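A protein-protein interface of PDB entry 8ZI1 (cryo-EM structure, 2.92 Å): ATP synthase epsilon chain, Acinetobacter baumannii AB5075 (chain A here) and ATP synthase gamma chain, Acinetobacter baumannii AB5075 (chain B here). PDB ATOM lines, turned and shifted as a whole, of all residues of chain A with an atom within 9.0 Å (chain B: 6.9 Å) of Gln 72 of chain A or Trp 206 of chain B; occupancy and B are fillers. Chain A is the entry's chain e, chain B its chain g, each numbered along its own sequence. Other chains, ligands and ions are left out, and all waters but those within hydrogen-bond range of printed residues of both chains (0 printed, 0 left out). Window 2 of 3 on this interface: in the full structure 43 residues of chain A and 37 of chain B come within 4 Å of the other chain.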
ATOM      1  N   ALA A   2     -18.735  -6.112 -37.808  1.00  0.00           N
ATOM      2  CA  ALA A   2     -20.007  -6.793 -37.595  1.00  0.00           C
ATOM      3  C   ALA A   2     -19.806  -8.302 -37.517  1.00  0.00           C
ATOM      4  O   ALA A   2     -19.550  -8.850 -36.445  1.00  0.00           O
ATOM      5  CB  ALA A   2     -20.990  -6.443 -38.701  1.00  0.00           C
ATOM      6  N   GLN A   5     -16.574 -14.193 -39.313  1.00  0.00           N
ATOM      7  CA  GLN A   5     -16.509 -15.629 -39.540  1.00  0.00           C
ATOM      8  C   GLN A   5     -17.361 -16.346 -38.504  1.00  0.00           C
ATOM      9  O   GLN A   5     -17.456 -15.920 -37.349  1.00  0.00           O
ATOM     10  CB  GLN A   5     -15.066 -16.151 -39.499  1.00  0.00           C
ATOM     11  CG  GLN A   5     -14.401 -16.077 -38.134  1.00  0.00           C
ATOM     12  CD  GLN A   5     -13.364 -14.975 -38.056  1.00  0.00           C
ATOM     13  OE1 GLN A   5     -13.230 -14.168 -38.975  1.00  0.00           O
ATOM     14  NE2 GLN A   5     -12.624 -14.935 -36.955  1.00  0.00           N
ATOM     15  N   CYS A   6     -17.985 -17.441 -38.941  1.00  0.00           N
ATOM     16  CA  CYS A   6     -18.778 -18.302 -38.065  1.00  0.00           C
ATOM     17  C   CYS A   6     -18.562 -19.730 -38.559  1.00  0.00           C
ATOM     18  O   CYS A   6     -19.117 -20.120 -39.590  1.00  0.00           O
ATOM     19  CB  CYS A   6     -20.251 -17.918 -38.087  1.00  0.00           C
ATOM     20  SG  CYS A   6     -20.619 -16.258 -37.469  1.00  0.00           S
ATOM     21  N   GLU A  31     -30.475 -16.746 -31.367  1.00  0.00           N
ATOM     22  CA  GLU A  31     -29.484 -15.810 -30.774  1.00  0.00           C
ATOM     23  C   GLU A  31     -28.521 -15.374 -31.873  1.00  0.00           C
ATOM     24  O   GLU A  31     -28.111 -14.195 -31.875  1.00  0.00           O
ATOM     25  CB  GLU A  31     -28.737 -16.506 -29.635  1.00  0.00           C
ATOM     26  CG  GLU A  31     -27.557 -15.717 -29.095  1.00  0.00           C
ATOM     27  CD  GLU A  31     -26.217 -16.037 -29.737  1.00  0.00           C
ATOM     28  OE1 GLU A  31     -26.119 -17.082 -30.410  1.00  0.00           O
ATOM     29  OE2 GLU A  31     -25.277 -15.235 -29.570  1.00  0.00           O
ATOM     30  N   LEU A  32     -28.192 -16.291 -32.780  1.00  0.00           N
ATOM     31  CA  LEU A  32     -27.219 -15.985 -33.857  1.00  0.00           C
ATOM     32  C   LEU A  32     -27.816 -14.954 -34.817  1.00  0.00           C
ATOM     33  O   LEU A  32     -29.040 -14.753 -34.789  1.00  0.00           O
ATOM     34  CB  LEU A  32     -26.844 -17.280 -34.581  1.00  0.00           C
ATOM     35  CG  LEU A  32     -26.097 -18.319 -33.750  1.00  0.00           C
ATOM     36  CD1 LEU A  32     -25.924 -19.600 -34.547  1.00  0.00           C
ATOM     37  CD2 LEU A  32     -24.740 -17.784 -33.314  1.00  0.00           C
ATOM     38  N   LEU A  35     -22.997 -10.580 -35.780  1.00  0.00           N
ATOM     39  CA  LEU A  35     -22.257 -11.006 -34.560  1.00  0.00           C
ATOM     40  C   LEU A  35     -22.573 -10.105 -33.370  1.00  0.00           C
ATOM     41  O   LEU A  35     -22.407  -8.875 -33.480  1.00  0.00           O
ATOM     42  CB  LEU A  35     -20.756 -10.969 -34.853  1.00  0.00           C
ATOM     43  CG  LEU A  35     -20.265 -11.957 -35.905  1.00  0.00           C
ATOM     44  CD1 LEU A  35     -18.793 -11.724 -36.212  1.00  0.00           C
ATOM     45  CD2 LEU A  35     -20.501 -13.379 -35.429  1.00  0.00           C
ATOM     46  N   PRO A  36     -23.012 -10.685 -32.234  1.00  0.00           N
ATOM     47  CA  PRO A  36     -23.240  -9.915 -31.010  1.00  0.00           C
ATOM     48  C   PRO A  36     -21.921  -9.402 -30.417  1.00  0.00           C
ATOM     49  O   PRO A  36     -21.873  -8.259 -30.012  1.00  0.00           O
ATOM     50  CB  PRO A  36     -23.862 -10.963 -30.073  1.00  0.00           C
ATOM     51  CG  PRO A  36     -24.373 -12.051 -30.986  1.00  0.00           C
ATOM     52  CD  PRO A  36     -23.345 -12.102 -32.091  1.00  0.00           C
ATOM     53  N   GLY A  37     -20.890 -10.252 -30.394  1.00  0.00           N
ATOM     54  CA  GLY A  37     -19.577  -9.868 -29.834  1.00  0.00           C
ATOM     55  C   GLY A  37     -19.658  -9.422 -28.383  1.00  0.00           C
ATOM     56  O   GLY A  37     -19.254  -8.275 -28.111  1.00  0.00           O
ATOM     57  N   HIS A  38     -20.121 -10.300 -27.481  1.00  0.00           N
ATOM     58  CA  HIS A  38     -20.243  -9.968 -26.035  1.00  0.00           C
ATOM     59  C   HIS A  38     -20.670 -11.214 -25.254  1.00  0.00           C
ATOM     60  O   HIS A  38     -20.923 -12.251 -25.902  1.00  0.00           O
ATOM     61  CB  HIS A  38     -21.216  -8.800 -25.810  1.00  0.00           C
ATOM     62  CG  HIS A  38     -21.360  -8.372 -24.388  1.00  0.00           C
ATOM     63  ND1 HIS A  38     -20.305  -7.876 -23.645  1.00  0.00           N
ATOM     64  CD2 HIS A  38     -22.439  -8.341 -23.575  1.00  0.00           C
ATOM     65  CE1 HIS A  38     -20.725  -7.573 -22.435  1.00  0.00           C
ATOM     66  NE2 HIS A  38     -22.030  -7.852 -22.365  1.00  0.00           N
ATOM     67  N   ALA A  39     -20.746 -11.111 -23.921  1.00  0.00           N
ATOM     68  CA  ALA A  39     -21.195 -12.253 -23.085  1.00  0.00           C
ATOM     69  C   ALA A  39     -20.732 -13.593 -23.674  1.00  0.00           C
ATOM     70  O   ALA A  39     -21.601 -14.450 -23.898  1.00  0.00           O
ATOM     71  CB  ALA A  39     -22.696 -12.217 -22.922  1.00  0.00           C
ATOM     72  N   PRO A  40     -19.430 -13.825 -23.953  1.00  0.00           N
ATOM     73  CA  PRO A  40     -18.990 -15.129 -24.446  1.00  0.00           C
ATOM     74  C   PRO A  40     -19.619 -16.265 -23.628  1.00  0.00           C
ATOM     75  O   PRO A  40     -19.641 -16.155 -22.416  1.00  0.00           O
ATOM     76  CB  PRO A  40     -17.475 -15.085 -24.222  1.00  0.00           C
ATOM     77  CG  PRO A  40     -17.145 -13.625 -24.388  1.00  0.00           C
ATOM     78  CD  PRO A  40     -18.307 -12.907 -23.740  1.00  0.00           C
ATOM     79  N   LEU A  41     -20.099 -17.320 -24.295  1.00  0.00           N
ATOM     80  CA  LEU A  41     -20.808 -18.406 -23.566  1.00  0.00           C
ATOM     81  C   LEU A  41     -20.797 -19.694 -24.387  1.00  0.00           C
ATOM     82  O   LEU A  41     -20.311 -19.649 -25.534  1.00  0.00           O
ATOM     83  CB  LEU A  41     -22.253 -17.975 -23.284  1.00  0.00           C
ATOM     84  CG  LEU A  41     -23.083 -17.566 -24.501  1.00  0.00           C
ATOM     85  CD1 LEU A  41     -23.859 -18.745 -25.066  1.00  0.00           C
ATOM     86  CD2 LEU A  41     -24.042 -16.441 -24.147  1.00  0.00           C
ATOM     87  N   VAL A  42     -21.331 -20.784 -23.825  1.00  0.00           N
ATOM     88  CA  VAL A  42     -21.400 -22.067 -24.512  1.00  0.00           C
ATOM     89  C   VAL A  42     -22.752 -22.699 -24.208  1.00  0.00           C
ATOM     90  O   VAL A  42     -23.225 -22.662 -23.067  1.00  0.00           O
ATOM     91  CB  VAL A  42     -20.240 -23.004 -24.108  1.00  0.00           C
ATOM     92  CG1 VAL A  42     -18.905 -22.383 -24.485  1.00  0.00           C
ATOM     93  CG2 VAL A  42     -20.273 -23.299 -22.614  1.00  0.00           C
ATOM     94  N   LEU A  69     -22.277 -24.964 -28.994  1.00  0.00           N
ATOM     95  CA  LEU A  69     -22.141 -23.634 -29.645  1.00  0.00           C
ATOM     96  C   LEU A  69     -21.414 -22.655 -28.718  1.00  0.00           C
ATOM     97  O   LEU A  69     -21.921 -22.423 -27.607  1.00  0.00           O
ATOM     98  CB  LEU A  69     -23.545 -23.126 -29.987  1.00  0.00           C
ATOM     99  CG  LEU A  69     -23.597 -21.858 -30.834  1.00  0.00           C
ATOM    100  CD1 LEU A  69     -24.805 -21.875 -31.757  1.00  0.00           C
ATOM    101  CD2 LEU A  69     -23.604 -20.614 -29.959  1.00  0.00           C
ATOM    102  N   GLU A  70     -20.293 -22.086 -29.173  1.00  0.00           N
ATOM    103  CA  GLU A  70     -19.539 -21.119 -28.389  1.00  0.00           C
ATOM    104  C   GLU A  70     -19.507 -19.797 -29.141  1.00  0.00           C
ATOM    105  O   GLU A  70     -19.263 -19.771 -30.352  1.00  0.00           O
ATOM    106  CB  GLU A  70     -18.112 -21.609 -28.117  1.00  0.00           C
ATOM    107  CG  GLU A  70     -17.266 -20.641 -27.305  1.00  0.00           C
ATOM    108  CD  GLU A  70     -16.418 -19.735 -28.176  1.00  0.00           C
ATOM    109  OE1 GLU A  70     -16.250 -20.045 -29.374  1.00  0.00           O
ATOM    110  OE2 GLU A  70     -15.920 -18.711 -27.663  1.00  0.00           O
ATOM    111  N   VAL A  71     -19.753 -18.708 -28.418  1.00  0.00           N
ATOM    112  CA  VAL A  71     -19.748 -17.365 -28.981  1.00  0.00           C
ATOM    113  C   VAL A  71     -18.755 -16.518 -28.195  1.00  0.00           C
ATOM    114  O   VAL A  71     -18.556 -16.729 -26.993  1.00  0.00           O
ATOM    115  CB  VAL A  71     -21.157 -16.734 -28.968  1.00  0.00           C
ATOM    116  CG1 VAL A  71     -21.604 -16.429 -27.548  1.00  0.00           C
ATOM    117  CG2 VAL A  71     -21.198 -15.483 -29.836  1.00  0.00           C
ATOM    118  N   GLN A  72     -18.120 -15.577 -28.887  1.00  0.00           N
ATOM    119  CA  GLN A  72     -17.121 -14.693 -28.307  1.00  0.00           C
ATOM    120  C   GLN A  72     -16.993 -13.504 -29.245  1.00  0.00           C
ATOM    121  O   GLN A  72     -17.337 -13.626 -30.425  1.00  0.00           O
ATOM    122  CB  GLN A  72     -15.777 -15.425 -28.147  1.00  0.00           C
ATOM    123  CG  GLN A  72     -14.677 -14.660 -27.426  1.00  0.00           C
ATOM    124  CD  GLN A  72     -13.756 -13.927 -28.380  1.00  0.00           C
ATOM    125  OE1 GLN A  72     -13.444 -14.423 -29.462  1.00  0.00           O
ATOM    126  NE2 GLN A  72     -13.323 -12.735 -27.987  1.00  0.00           N
ATOM    127  N   PRO A  73     -16.560 -12.336 -28.753  1.00  0.00           N
ATOM    128  CA  PRO A  73     -16.304 -11.216 -29.667  1.00  0.00           C
ATOM    129  C   PRO A  73     -15.454 -11.608 -30.867  1.00  0.00           C
ATOM    130  O   PRO A  73     -14.290 -11.994 -30.720  1.00  0.00           O
ATOM    131  CB  PRO A  73     -15.584 -10.204 -28.770  1.00  0.00           C
ATOM    132  CG  PRO A  73     -16.198 -10.429 -27.425  1.00  0.00           C
ATOM    133  CD  PRO A  73     -16.606 -11.888 -27.348  1.00  0.00           C
ATOM    134  N   HIS A  74     -16.054 -11.524 -32.057  1.00  0.00           N
ATOM    135  CA  HIS A  74     -15.449 -11.812 -33.356  1.00  0.00           C
ATOM    136  C   HIS A  74     -15.197 -13.296 -33.598  1.00  0.00           C
ATOM    137  O   HIS A  74     -14.470 -13.642 -34.538  1.00  0.00           O
ATOM    138  CB  HIS A  74     -14.135 -11.043 -33.563  1.00  0.00           C
ATOM    139  CG  HIS A  74     -14.225  -9.587 -33.225  1.00  0.00           C
ATOM    140  ND1 HIS A  74     -14.546  -8.624 -34.157  1.00  0.00           N
ATOM    141  CD2 HIS A  74     -14.032  -8.930 -32.057  1.00  0.00           C
ATOM    142  CE1 HIS A  74     -14.549  -7.436 -33.578  1.00  0.00           C
ATOM    143  NE2 HIS A  74     -14.240  -7.594 -32.304  1.00  0.00           N
ATOM    144  N   VAL A  75     -15.773 -14.187 -32.792  1.00  0.00           N
ATOM    145  CA  VAL A  75     -15.571 -15.625 -32.950  1.00  0.00           C
ATOM    146  C   VAL A  75     -16.888 -16.348 -32.692  1.00  0.00           C
ATOM    147  O   VAL A  75     -17.540 -16.121 -31.668  1.00  0.00           O
ATOM    148  CB  VAL A  75     -14.472 -16.156 -32.005  1.00  0.00           C
ATOM    149  CG1 VAL A  75     -14.612 -17.658 -31.808  1.00  0.00           C
ATOM    150  CG2 VAL A  75     -13.092 -15.814 -32.547  1.00  0.00           C
ATOM    151  N   VAL A  76     -17.281 -17.215 -33.622  1.00  0.00           N
ATOM    152  CA  VAL A  76     -18.423 -18.106 -33.445  1.00  0.00           C
ATOM    153  C   VAL A  76     -17.993 -19.503 -33.868  1.00  0.00           C
ATOM    154  O   VAL A  76     -17.593 -19.709 -35.021  1.00  0.00           O
ATOM    155  CB  VAL A  76     -19.651 -17.651 -34.252  1.00  0.00           C
ATOM    156  CG1 VAL A  76     -20.790 -18.644 -34.084  1.00  0.00           C
ATOM    157  CG2 VAL A  76     -20.088 -16.261 -33.819  1.00  0.00           C
ATOM    158  N   THR A  77     -18.079 -20.462 -32.946  1.00  0.00           N
ATOM    159  CA  THR A  77     -17.643 -21.826 -33.205  1.00  0.00           C
ATOM    160  C   THR A  77     -18.764 -22.799 -32.873  1.00  0.00           C
ATOM    161  O   THR A  77     -19.470 -22.632 -31.876  1.00  0.00           O
ATOM    162  CB  THR A  77     -16.394 -22.177 -32.389  1.00  0.00           C
ATOM    163  OG1 THR A  77     -16.556 -21.719 -31.041  1.00  0.00           O
ATOM    164  CG2 THR A  77     -15.162 -21.524 -32.996  1.00  0.00           C
ATOM    165  N   HIS B  55      -9.202 -23.761 -23.893  1.00  0.00           N
ATOM    166  CA  HIS B  55      -9.910 -22.563 -23.459  1.00  0.00           C
ATOM    167  C   HIS B  55     -10.819 -22.857 -22.273  1.00  0.00           C
ATOM    168  O   HIS B  55     -10.866 -22.082 -21.313  1.00  0.00           O
ATOM    169  CB  HIS B  55     -10.713 -21.971 -24.616  1.00  0.00           C
ATOM    170  CG  HIS B  55     -11.080 -20.533 -24.417  1.00  0.00           C
ATOM    171  ND1 HIS B  55     -12.136 -20.137 -23.626  1.00  0.00           N
ATOM    172  CD2 HIS B  55     -10.525 -19.397 -24.901  1.00  0.00           C
ATOM    173  CE1 HIS B  55     -12.219 -18.818 -23.634  1.00  0.00           C
ATOM    174  NE2 HIS B  55     -11.253 -18.345 -24.401  1.00  0.00           N
ATOM    175  N   ALA B  59     -10.526 -21.594 -18.491  1.00  0.00           N
ATOM    176  CA  ALA B  59     -11.651 -20.795 -18.022  1.00  0.00           C
ATOM    177  C   ALA B  59     -12.087 -21.205 -16.622  1.00  0.00           C
ATOM    178  O   ALA B  59     -12.314 -20.344 -15.764  1.00  0.00           O
ATOM    179  CB  ALA B  59     -12.816 -20.907 -19.003  1.00  0.00           C
ATOM    180  N   ARG B 202      -2.719 -13.567 -23.754  1.00  0.00           N
ATOM    181  CA  ARG B 202      -3.498 -12.602 -24.578  1.00  0.00           C
ATOM    182  C   ARG B 202      -4.978 -12.620 -24.181  1.00  0.00           C
ATOM    183  O   ARG B 202      -5.735 -13.420 -24.764  1.00  0.00           O
ATOM    184  CB  ARG B 202      -3.324 -12.916 -26.069  1.00  0.00           C
ATOM    185  CG  ARG B 202      -3.408 -14.396 -26.413  1.00  0.00           C
ATOM    186  CD  ARG B 202      -3.554 -14.626 -27.904  1.00  0.00           C
ATOM    187  NE  ARG B 202      -4.148 -15.920 -28.205  1.00  0.00           N
ATOM    188  CZ  ARG B 202      -3.466 -17.053 -28.314  1.00  0.00           C
ATOM    189  NH1 ARG B 202      -2.154 -17.056 -28.147  1.00  0.00           N
ATOM    190  NH2 ARG B 202      -4.096 -18.180 -28.591  1.00  0.00           N
ATOM    191  N   THR B 203      -5.367 -11.764 -23.227  1.00  0.00           N
ATOM    192  CA  THR B 203      -6.789 -11.653 -22.782  1.00  0.00           C
ATOM    193  C   THR B 203      -7.377 -13.057 -22.541  1.00  0.00           C
ATOM    194  O   THR B 203      -6.721 -13.834 -21.819  1.00  0.00           O
ATOM    195  CB  THR B 203      -7.575 -10.728 -23.728  1.00  0.00           C
ATOM    196  OG1 THR B 203      -7.771 -11.416 -24.963  1.00  0.00           O
ATOM    197  CG2 THR B 203      -6.876  -9.410 -23.979  1.00  0.00           C
ATOM    198  N   TYR B 204      -8.562 -13.364 -23.088  1.00  0.00           N
ATOM    199  CA  TYR B 204      -9.231 -14.666 -22.821  1.00  0.00           C
ATOM    200  C   TYR B 204      -9.392 -14.834 -21.307  1.00  0.00           C
ATOM    201  O   TYR B 204      -9.210 -15.962 -20.808  1.00  0.00           O
ATOM    202  CB  TYR B 204      -8.452 -15.820 -23.456  1.00  0.00           C
ATOM    203  CG  TYR B 204      -8.440 -15.804 -24.963  1.00  0.00           C
ATOM    204  CD1 TYR B 204      -9.608 -15.620 -25.683  1.00  0.00           C
ATOM    205  CD2 TYR B 204      -7.262 -15.972 -25.671  1.00  0.00           C
ATOM    206  CE1 TYR B 204      -9.608 -15.603 -27.068  1.00  0.00           C
ATOM    207  CE2 TYR B 204      -7.244 -15.956 -27.056  1.00  0.00           C
ATOM    208  CZ  TYR B 204      -8.421 -15.772 -27.757  1.00  0.00           C
ATOM    209  OH  TYR B 204      -8.410 -15.756 -29.121  1.00  0.00           O
ATOM    210  N   GLY B 205      -9.758 -13.756 -20.609  1.00  0.00           N
ATOM    211  CA  GLY B 205     -10.022 -13.850 -19.160  1.00  0.00           C
ATOM    212  C   GLY B 205     -11.516 -13.812 -18.888  1.00  0.00           C
ATOM    213  O   GLY B 205     -11.923 -14.188 -17.771  1.00  0.00           O
ATOM    214  N   TRP B 206     -12.306 -13.381 -19.877  1.00  0.00           N
ATOM    215  CA  TRP B 206     -13.786 -13.312 -19.729  1.00  0.00           C
ATOM    216  C   TRP B 206     -14.356 -14.717 -19.522  1.00  0.00           C
ATOM    217  O   TRP B 206     -15.338 -14.841 -18.762  1.00  0.00           O
ATOM    218  CB  TRP B 206     -14.415 -12.628 -20.950  1.00  0.00           C
ATOM    219  CG  TRP B 206     -13.900 -13.140 -22.259  1.00  0.00           C
ATOM    220  CD1 TRP B 206     -14.307 -14.259 -22.926  1.00  0.00           C
ATOM    221  CD2 TRP B 206     -12.870 -12.546 -23.069  1.00  0.00           C
ATOM    222  NE1 TRP B 206     -13.604 -14.404 -24.091  1.00  0.00           N
ATOM    223  CE2 TRP B 206     -12.716 -13.367 -24.206  1.00  0.00           C
ATOM    224  CE3 TRP B 206     -12.067 -11.408 -22.945  1.00  0.00           C
ATOM    225  CZ2 TRP B 206     -11.791 -13.081 -25.209  1.00  0.00           C
ATOM    226  CZ3 TRP B 206     -11.156 -11.126 -23.937  1.00  0.00           C
ATOM    227  CH2 TRP B 206     -11.022 -11.952 -25.053  1.00  0.00           C
ATOM    228  N   ASP B 207     -13.779 -15.723 -20.188  1.00  0.00           N
ATOM    229  CA  ASP B 207     -14.296 -17.116 -20.100  1.00  0.00           C
ATOM    230  C   ASP B 207     -15.733 -17.149 -20.634  1.00  0.00           C
ATOM    231  O   ASP B 207     -15.977 -16.528 -21.685  1.00  0.00           O
ATOM    232  CB  ASP B 207     -14.184 -17.663 -18.673  1.00  0.00           C
ATOM    233  CG  ASP B 207     -12.824 -17.412 -18.045  1.00  0.00           C
ATOM    234  OD1 ASP B 207     -11.854 -17.224 -18.807  1.00  0.00           O
ATOM    235  OD2 ASP B 207     -12.745 -17.402 -16.802  1.00  0.00           O
ATOM    236  N   TYR B 208     -16.643 -17.840 -19.941  1.00  0.00           N
ATOM    237  CA  TYR B 208     -18.034 -17.978 -20.452  1.00  0.00           C
ATOM    238  C   TYR B 208     -19.042 -17.750 -19.322  1.00  0.00           C
ATOM    239  O   TYR B 208     -18.739 -18.101 -18.167  1.00  0.00           O
ATOM    240  CB  TYR B 208     -18.237 -19.353 -21.091  1.00  0.00           C
ATOM    241  CG  TYR B 208     -17.278 -19.658 -22.213  1.00  0.00           C
ATOM    242  CD1 TYR B 208     -17.274 -18.900 -23.371  1.00  0.00           C
ATOM    243  CD2 TYR B 208     -16.364 -20.694 -22.113  1.00  0.00           C
ATOM    244  CE1 TYR B 208     -16.390 -19.163 -24.403  1.00  0.00           C
ATOM    245  CE2 TYR B 208     -15.476 -20.974 -23.137  1.00  0.00           C
ATOM    246  CZ  TYR B 208     -15.490 -20.206 -24.287  1.00  0.00           C
ATOM    247  OH  TYR B 208     -14.619 -20.475 -25.303  1.00  0.00           O
ATOM    248  N   ILE B 209     -20.223 -17.241 -19.668  1.00  0.00           N
ATOM    249  CA  ILE B 209     -21.284 -17.111 -18.633  1.00  0.00           C
ATOM    250  C   ILE B 209     -21.748 -18.525 -18.269  1.00  0.00           C
ATOM    251  O   ILE B 209     -22.379 -18.675 -17.205  1.00  0.00           O
ATOM    252  CB  ILE B 209     -22.434 -16.221 -19.141  1.00  0.00           C
ATOM    253  CG1 ILE B 209     -23.364 -16.970 -20.098  1.00  0.00           C
ATOM    254  CG2 ILE B 209     -21.890 -14.948 -19.772  1.00  0.00           C
ATOM    255  CD1 ILE B 209     -24.538 -16.146 -20.565  1.00  0.00           C
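O of Pro 40 of chain A sits at hydrogen-bond distance from N of Ile 209 of chain B, at 3.0 Å.
OH of Tyr 208 of chain B sits at hydrogen-bond distance from OE2 of Glu 70 of chain A (3.2 Å).
The backbone NH (N) of Val 71 of chain A lies within hydrogen-bond range of the backbone carbonyl oxygen (O) of Leu 41 of chain A, at 3.1 Å.
A ring nitrogen (ND1) of His 55 of chain B is in hydrogen-bond range of the side-chain hydroxyl (OH) of Tyr 208 of chain B.
O of Thr 77 of chain A is in hydrogen-bond range of N of Glu 70 of chain A, at 2.9 Å.
Pro 40 of chain A touches Trp 206 of chain B.
Pro 40 of chain A touches Asp 207 of chain B (CB to O, 3.3 Å).
O of Pro 40 of chain A touches CA of Tyr 208 of chain B, 3.1 Å away.
Tyr 208 of chain B touches Leu 41 of chain A.
Ile 209 of chain B touches Leu 41 of chain A.
CD2 of Tyr 208 of chain B touches CG1 of Val 42 of chain A, at 3.9 Å.
Gln 72 of chain A touches Trp 206 of chain B (NE2 to CZ2, 3.2 Å).
Gln 5 of chain A touches none of the printed residues of chain B.
Of the printed residues of chain B, Pro 40 of chain A touches Trp 206 (3.3 Å), Asp 207 (3.3 Å), Tyr 208 (3.1 Å) and Ile 209 (3.0 Å).
Printed residues of chain B within 4 Å of Val 42 of chain A: Tyr 208 (3.9 Å).
Val 71 of chain A touches none of the printed residues of chain B.
Gln 72 of chain A touches just one residue of chain B: Trp 206 (3.2 Å).
No residue of chain A comes within 4 Å of Gly 205 of chain B.
Of chain A, only Pro 40 and Gln 72 come within 4 Å of Trp 206 of chain B.
Printed residues of chain A within 4 Å of Asp 207 of chain B: Pro 40 (3.3 Å).
Of the printed residues of chain A, Tyr 208 of chain B touches Pro 40, Leu 41, Val 42 and Glu 70.
The nearest residue of chain B that does not touch Gln 72 of chain A is Tyr 204 of chain B (4.7 Å).
The nearest residue of chain A that does not touch Trp 206 of chain B is Pro 73 of chain A (5.1 Å).
The nearest printed residue of chain B that does not touch Glu 70 of chain A is His 55 of chain B (5.5 Å).
Of the 10 printed residues of chain B, 4 touch a printed residue of chain A.
Hydrophobic or aromatic side chains of chain B within 4 Å of the printed part of chain A: Trp 206, Tyr 208 and Ile 209.
Of the 22 printed residues of chain A, 5 touch a printed residue of chain B.
Printed residues of chain A that touch a printed residue of chain B: Pro 40, Leu 41, Val 42, Glu 70 and Gln 72.
Hydrophobic or aromatic side chains of chain A that line the printed part of chain B: Pro 40, Leu 41 and Val 42.
Along chain A the printed residues that touch a printed residue of chain B span positions 40 to 72.
Among the printed residues, no Asp or Glu carboxylate lies within 4 Å of a Lys or Arg side-chain nitrogen of the other chain.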
